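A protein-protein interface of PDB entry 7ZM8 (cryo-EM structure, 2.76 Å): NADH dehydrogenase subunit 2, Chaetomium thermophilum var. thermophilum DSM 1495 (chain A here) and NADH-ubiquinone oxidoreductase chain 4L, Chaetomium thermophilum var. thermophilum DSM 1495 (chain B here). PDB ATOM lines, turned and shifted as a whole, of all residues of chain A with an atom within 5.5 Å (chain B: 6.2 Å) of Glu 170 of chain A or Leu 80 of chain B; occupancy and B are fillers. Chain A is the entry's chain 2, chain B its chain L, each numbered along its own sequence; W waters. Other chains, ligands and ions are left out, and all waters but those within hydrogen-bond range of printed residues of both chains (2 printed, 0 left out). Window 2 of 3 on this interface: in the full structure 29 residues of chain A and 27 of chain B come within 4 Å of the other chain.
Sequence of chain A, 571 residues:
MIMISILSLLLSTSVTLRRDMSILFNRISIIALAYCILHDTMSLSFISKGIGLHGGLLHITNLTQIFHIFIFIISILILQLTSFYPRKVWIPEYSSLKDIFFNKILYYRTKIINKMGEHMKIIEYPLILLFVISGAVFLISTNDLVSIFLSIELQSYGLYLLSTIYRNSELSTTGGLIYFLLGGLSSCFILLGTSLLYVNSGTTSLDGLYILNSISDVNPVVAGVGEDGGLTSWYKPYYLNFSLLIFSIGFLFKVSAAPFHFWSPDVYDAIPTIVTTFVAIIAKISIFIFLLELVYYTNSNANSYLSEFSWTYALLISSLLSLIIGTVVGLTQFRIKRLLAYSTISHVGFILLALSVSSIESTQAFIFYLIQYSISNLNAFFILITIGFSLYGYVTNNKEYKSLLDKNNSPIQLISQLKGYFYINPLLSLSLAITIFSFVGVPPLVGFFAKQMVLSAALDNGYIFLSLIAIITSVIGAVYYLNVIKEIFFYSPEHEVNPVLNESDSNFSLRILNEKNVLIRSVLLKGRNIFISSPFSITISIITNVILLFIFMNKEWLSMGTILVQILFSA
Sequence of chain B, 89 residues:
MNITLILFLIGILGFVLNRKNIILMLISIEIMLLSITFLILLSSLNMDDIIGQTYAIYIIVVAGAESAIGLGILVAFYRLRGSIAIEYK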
ATOM      1  N   ARG A 167     -18.993 -22.653  -1.063  1.00  0.00           N
ATOM      2  CA  ARG A 167     -18.509 -23.157  -2.377  1.00  0.00           C
ATOM      3  C   ARG A 167     -17.233 -22.449  -2.821  1.00  0.00           C
ATOM      4  O   ARG A 167     -16.533 -23.015  -3.668  1.00  0.00           O
ATOM      5  CB  ARG A 167     -19.640 -23.070  -3.406  1.00  0.00           C
ATOM      6  CG  ARG A 167     -20.312 -21.711  -3.512  1.00  0.00           C
ATOM      7  CD  ARG A 167     -21.522 -21.758  -4.426  1.00  0.00           C
ATOM      8  NE  ARG A 167     -21.222 -22.243  -5.766  1.00  0.00           N
ATOM      9  CZ  ARG A 167     -20.901 -21.471  -6.798  1.00  0.00           C
ATOM     10  NH1 ARG A 167     -20.648 -22.015  -7.974  1.00  0.00           N
ATOM     11  NH2 ARG A 167     -20.836 -20.160  -6.655  1.00  0.00           N
ATOM     12  N   ASN A 168     -16.942 -21.268  -2.281  1.00  0.00           N
ATOM     13  CA  ASN A 168     -15.757 -20.523  -2.777  1.00  0.00           C
ATOM     14  C   ASN A 168     -14.544 -20.945  -1.955  1.00  0.00           C
ATOM     15  O   ASN A 168     -13.434 -20.513  -2.288  1.00  0.00           O
ATOM     16  CB  ASN A 168     -16.011 -19.020  -2.862  1.00  0.00           C
ATOM     17  CG  ASN A 168     -17.110 -18.653  -3.837  1.00  0.00           C
ATOM     18  OD1 ASN A 168     -17.730 -19.525  -4.438  1.00  0.00           O
ATOM     19  ND2 ASN A 168     -17.359 -17.366  -4.000  1.00  0.00           N
ATOM     20  N   SER A 169     -14.761 -21.776  -0.932  1.00  0.00           N
ATOM     21  CA  SER A 169     -13.651 -22.285  -0.090  1.00  0.00           C
ATOM     22  C   SER A 169     -13.116 -23.596  -0.661  1.00  0.00           C
ATOM     23  O   SER A 169     -13.914 -24.527  -0.836  1.00  0.00           O
ATOM     24  CB  SER A 169     -14.074 -22.441   1.332  1.00  0.00           C
ATOM     25  OG  SER A 169     -13.053 -23.058   2.098  1.00  0.00           O
ATOM     26  N   GLU A 170     -11.820 -23.646  -0.965  1.00  0.00           N
ATOM     27  CA  GLU A 170     -11.177 -24.866  -1.493  1.00  0.00           C
ATOM     28  C   GLU A 170     -10.890 -25.797  -0.321  1.00  0.00           C
ATOM     29  O   GLU A 170     -10.522 -26.938  -0.555  1.00  0.00           O
ATOM     30  CB  GLU A 170      -9.906 -24.475  -2.236  1.00  0.00           C
ATOM     31  CG  GLU A 170     -10.087 -23.280  -3.151  1.00  0.00           C
ATOM     32  CD  GLU A 170      -8.970 -23.077  -4.160  1.00  0.00           C
ATOM     33  OE1 GLU A 170      -7.904 -23.697  -3.990  1.00  0.00           O
ATOM     34  OE2 GLU A 170      -9.174 -22.305  -5.122  1.00  0.00           O
ATOM     35  N   LEU A 171     -11.127 -25.338   0.901  1.00  0.00           N
ATOM     36  CA  LEU A 171     -10.954 -26.205   2.085  1.00  0.00           C
ATOM     37  C   LEU A 171     -12.289 -26.869   2.369  1.00  0.00           C
ATOM     38  O   LEU A 171     -12.285 -28.041   2.751  1.00  0.00           O
ATOM     39  CB  LEU A 171     -10.473 -25.375   3.275  1.00  0.00           C
ATOM     40  CG  LEU A 171      -8.974 -25.102   3.320  1.00  0.00           C
ATOM     41  CD1 LEU A 171      -8.606 -24.415   4.619  1.00  0.00           C
ATOM     42  CD2 LEU A 171      -8.193 -26.391   3.156  1.00  0.00           C
ATOM     43  N   SER A 172     -13.391 -26.155   2.173  1.00  0.00           N
ATOM     44  CA  SER A 172     -14.714 -26.724   2.516  1.00  0.00           C
ATOM     45  C   SER A 172     -15.110 -27.768   1.474  1.00  0.00           C
ATOM     46  O   SER A 172     -15.701 -28.785   1.857  1.00  0.00           O
ATOM     47  CB  SER A 172     -15.735 -25.630   2.665  1.00  0.00           C
ATOM     48  OG  SER A 172     -15.284 -24.661   3.595  1.00  0.00           O
ATOM     49  N   THR A 173     -14.802 -27.514   0.207  1.00  0.00           N
ATOM     50  CA  THR A 173     -15.167 -28.449  -0.891  1.00  0.00           C
ATOM     51  C   THR A 173     -14.400 -29.758  -0.705  1.00  0.00           C
ATOM     52  O   THR A 173     -14.974 -30.813  -0.976  1.00  0.00           O
ATOM     53  CB  THR A 173     -15.006 -27.758  -2.252  1.00  0.00           C
ATOM     54  OG1 THR A 173     -13.683 -27.226  -2.302  1.00  0.00           O
ATOM     55  CG2 THR A 173     -16.015 -26.654  -2.470  1.00  0.00           C
ATOM     56  N   THR A 174     -13.139 -29.670  -0.286  1.00  0.00           N
ATOM     57  CA  THR A 174     -12.300 -30.865  -0.028  1.00  0.00           C
ATOM     58  C   THR A 174     -12.889 -31.646   1.137  1.00  0.00           C
ATOM     59  O   THR A 174     -13.043 -32.866   1.000  1.00  0.00           O
ATOM     60  CB  THR A 174     -10.925 -30.399   0.445  1.00  0.00           C
ATOM     61  OG1 THR A 174     -10.422 -29.523  -0.559  1.00  0.00           O
ATOM     62  CG2 THR A 174      -9.958 -31.530   0.706  1.00  0.00           C
ATOM     63  N   ASP A 406      -8.198 -19.458   4.303  1.00  0.00           N
ATOM     64  CA  ASP A 406      -9.614 -19.312   4.638  1.00  0.00           C
ATOM     65  C   ASP A 406      -9.789 -18.619   5.983  1.00  0.00           C
ATOM     66  O   ASP A 406     -10.531 -19.073   6.855  1.00  0.00           O
ATOM     67  CB  ASP A 406     -10.323 -20.666   4.621  1.00  0.00           C
ATOM     68  CG  ASP A 406     -10.732 -21.091   3.225  1.00  0.00           C
ATOM     69  OD1 ASP A 406     -11.428 -20.312   2.544  1.00  0.00           O
ATOM     70  OD2 ASP A 406     -10.356 -22.204   2.805  1.00  0.00           O
ATOM     71  N   VAL B  75     -18.234 -31.819  -8.472  1.00  0.00           N
ATOM     72  CA  VAL B  75     -18.192 -30.670  -9.369  1.00  0.00           C
ATOM     73  C   VAL B  75     -17.727 -29.429  -8.625  1.00  0.00           C
ATOM     74  O   VAL B  75     -16.907 -28.656  -9.131  1.00  0.00           O
ATOM     75  CB  VAL B  75     -19.565 -30.457 -10.031  1.00  0.00           C
ATOM     76  CG1 VAL B  75     -19.639 -29.088 -10.669  1.00  0.00           C
ATOM     77  CG2 VAL B  75     -19.819 -31.526 -11.061  1.00  0.00           C
ATOM     78  N   ALA B  76     -18.193 -29.238  -7.395  1.00  0.00           N
ATOM     79  CA  ALA B  76     -17.755 -28.096  -6.562  1.00  0.00           C
ATOM     80  C   ALA B  76     -16.245 -28.175  -6.328  1.00  0.00           C
ATOM     81  O   ALA B  76     -15.572 -27.121  -6.399  1.00  0.00           O
ATOM     82  CB  ALA B  76     -18.524 -28.121  -5.273  1.00  0.00           C
ATOM     83  N   PHE B  77     -15.730 -29.366  -6.038  1.00  0.00           N
ATOM     84  CA  PHE B  77     -14.281 -29.589  -5.822  1.00  0.00           C
ATOM     85  C   PHE B  77     -13.464 -29.309  -7.088  1.00  0.00           C
ATOM     86  O   PHE B  77     -12.452 -28.605  -6.988  1.00  0.00           O
ATOM     87  CB  PHE B  77     -14.115 -31.023  -5.318  1.00  0.00           C
ATOM     88  CG  PHE B  77     -12.708 -31.501  -5.089  1.00  0.00           C
ATOM     89  CD1 PHE B  77     -12.026 -31.167  -3.934  1.00  0.00           C
ATOM     90  CD2 PHE B  77     -12.084 -32.319  -6.016  1.00  0.00           C
ATOM     91  CE1 PHE B  77     -10.738 -31.624  -3.721  1.00  0.00           C
ATOM     92  CE2 PHE B  77     -10.795 -32.773  -5.802  1.00  0.00           C
ATOM     93  CZ  PHE B  77     -10.130 -32.428  -4.653  1.00  0.00           C
ATOM     94  N   TYR B  78     -13.913 -29.795  -8.246  1.00  0.00           N
ATOM     95  CA  TYR B  78     -13.209 -29.604  -9.542  1.00  0.00           C
ATOM     96  C   TYR B  78     -13.136 -28.128  -9.943  1.00  0.00           C
ATOM     97  O   TYR B  78     -12.109 -27.739 -10.499  1.00  0.00           O
ATOM     98  CB  TYR B  78     -13.880 -30.458 -10.624  1.00  0.00           C
ATOM     99  CG  TYR B  78     -13.202 -30.411 -11.966  1.00  0.00           C
ATOM    100  CD1 TYR B  78     -12.022 -31.096 -12.193  1.00  0.00           C
ATOM    101  CD2 TYR B  78     -13.740 -29.675 -13.005  1.00  0.00           C
ATOM    102  CE1 TYR B  78     -11.384 -31.042 -13.418  1.00  0.00           C
ATOM    103  CE2 TYR B  78     -13.117 -29.612 -14.237  1.00  0.00           C
ATOM    104  CZ  TYR B  78     -11.936 -30.299 -14.443  1.00  0.00           C
ATOM    105  OH  TYR B  78     -11.325 -30.237 -15.660  1.00  0.00           O
ATOM    106  N   ARG B  79     -14.177 -27.342  -9.675  1.00  0.00           N
ATOM    107  CA  ARG B  79     -14.235 -25.930 -10.119  1.00  0.00           C
ATOM    108  C   ARG B  79     -13.030 -25.186  -9.544  1.00  0.00           C
ATOM    109  O   ARG B  79     -12.493 -24.311 -10.242  1.00  0.00           O
ATOM    110  CB  ARG B  79     -15.533 -25.282  -9.622  1.00  0.00           C
ATOM    111  CG  ARG B  79     -15.734 -23.832 -10.037  1.00  0.00           C
ATOM    112  CD  ARG B  79     -17.087 -23.290  -9.628  1.00  0.00           C
ATOM    113  NE  ARG B  79     -17.136 -22.871  -8.238  1.00  0.00           N
ATOM    114  CZ  ARG B  79     -17.081 -21.611  -7.828  1.00  0.00           C
ATOM    115  NH1 ARG B  79     -17.127 -21.329  -6.538  1.00  0.00           N
ATOM    116  NH2 ARG B  79     -16.999 -20.633  -8.708  1.00  0.00           N
ATOM    117  N   LEU B  80     -12.650 -25.491  -8.301  1.00  0.00           N
ATOM    118  CA  LEU B  80     -11.528 -24.779  -7.650  1.00  0.00           C
ATOM    119  C   LEU B  80     -10.193 -25.520  -7.784  1.00  0.00           C
ATOM    120  O   LEU B  80      -9.163 -24.857  -7.651  1.00  0.00           O
ATOM    121  CB  LEU B  80     -11.901 -24.552  -6.186  1.00  0.00           C
ATOM    122  CG  LEU B  80     -13.242 -23.864  -5.943  1.00  0.00           C
ATOM    123  CD1 LEU B  80     -13.536 -23.790  -4.456  1.00  0.00           C
ATOM    124  CD2 LEU B  80     -13.265 -22.477  -6.562  1.00  0.00           C
ATOM    125  N   ARG B  81     -10.188 -26.822  -8.052  1.00  0.00           N
ATOM    126  CA  ARG B  81      -8.908 -27.582  -8.039  1.00  0.00           C
ATOM    127  C   ARG B  81      -8.395 -27.833  -9.459  1.00  0.00           C
ATOM    128  O   ARG B  81      -7.179 -27.727  -9.667  1.00  0.00           O
ATOM    129  CB  ARG B  81      -9.036 -28.845  -7.180  1.00  0.00           C
ATOM    130  CG  ARG B  81      -7.712 -29.490  -6.810  1.00  0.00           C
ATOM    131  CD  ARG B  81      -7.834 -30.136  -5.451  1.00  0.00           C
ATOM    132  NE  ARG B  81      -6.663 -30.884  -5.020  1.00  0.00           N
ATOM    133  CZ  ARG B  81      -5.739 -30.425  -4.186  1.00  0.00           C
ATOM    134  NH1 ARG B  81      -5.847 -29.210  -3.678  1.00  0.00           N
ATOM    135  NH2 ARG B  81      -4.713 -31.188  -3.855  1.00  0.00           N
ATOM    136  N   GLY B  82      -9.279 -28.153 -10.397  1.00  0.00           N
ATOM    137  CA  GLY B  82      -8.875 -28.324 -11.806  1.00  0.00           C
ATOM    138  C   GLY B  82      -8.391 -29.713 -12.109  1.00  0.00           C
ATOM    139  O   GLY B  82      -8.004 -29.961 -13.247  1.00  0.00           O
HETATM  140  O   HOH W   1     -11.535 -27.558  -4.284  1.00  0.00           O
HETATM  141  O   HOH W   2      -8.558 -29.549  -2.354  1.00  0.00           O
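NH1 of Arg 79 of chain B is in hydrogen-bond range of OD1 of Asn 168 of chain A (2.8 Å).
The backbone carbonyl oxygen (O) of Arg 167 of chain A sits at hydrogen-bond distance from the guanidinium group (NH1) of Arg 79 of chain B (3.4 Å).
OG1 of Thr 174 of chain A is in hydrogen-bond range of O of Glu 170 of chain A, 2.6 Å away.
The side-chain hydroxyl (OG) of Ser 169 of chain A lies within hydrogen-bond range of the backbone NH (N) of Ser 172 of chain A (3.1 Å).
OD2 of Asp 406 of chain A lies within hydrogen-bond range of OG of Ser 169 of chain A (2.9 Å).
The backbone carbonyl oxygen of Ser 169 of chain A sits at hydrogen-bond distance from the side-chain hydroxyl of Thr 173 of chain A.
The side-chain hydroxyl (OG) of Ser 169 of chain A lies close to the backbone NH (N) of Leu 171 of chain A.
O of Arg 167 of chain A touches CD1 of Leu 80 of chain B, at 3.2 Å.
Asn 168 of chain A touches Leu 80 of chain B.
Ser 169 of chain A touches Leu 80 of chain B.
Leu 80 of chain B touches Glu 170 of chain A.
Ala 76 of chain B touches Thr 173 of chain A.
CE1 of Phe 77 of chain B touches OG1 of Thr 174 of chain A, at 3.8 Å.
Leu 80 of chain B touches just these residues of chain A: Arg 167 (3.2 Å), Asn 168 (3.9 Å), Ser 169 (3.7 Å) and Glu 170 (3.6 Å).
Of the printed residues of chain B, Arg 167 of chain A touches Arg 79 and Leu 80.
Of the printed residues of chain B, Ser 169 of chain A touches Leu 80 (3.7 Å).
Printed residues of chain A within 4 Å of Arg 79 of chain B: Arg 167 (3.4 Å) and Asn 168 (2.8 Å).
Printed residues of chain A within 4 Å of Ala 76 of chain B: Thr 173 (3.98 Å).
Val 75 of chain B touches none of the printed residues of chain A.
The nearest residue of chain B that does not touch Glu 170 of chain A is Arg 81 of chain B (5.5 Å).
The nearest printed residue of chain B that does not touch Thr 174 of chain A is Arg 81 of chain B (5.5 Å).
Of the 8 printed residues of chain B, 4 touch a printed residue of chain A.
Printed residues of chain B that touch a printed residue of chain A: Ala 76, Phe 77, Arg 79 and Leu 80.
Hydrophobic or aromatic side chains of chain B within 4 Å of the printed part of chain A: Phe 77 and Leu 80.
Of the 9 printed residues of chain A, 6 touch a printed residue of chain B.
Along chain A the printed residues that touch a printed residue of chain B span positions 167 to 174.
Among the printed residues, no Asp or Glu carboxylate lies within 4 Å of a Lys or Arg side-chain nitrogen of the other chain.
Water W2 bridges OG1 of Thr 174 of chain A and NH1 of Arg 81 of chain B.
Water W1 lies within hydrogen-bond range of the side-chain hydroxyl (OG1) of Thr 173 of chain A and the backbone carbonyl oxygen (O) of Phe 77 of chain B.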
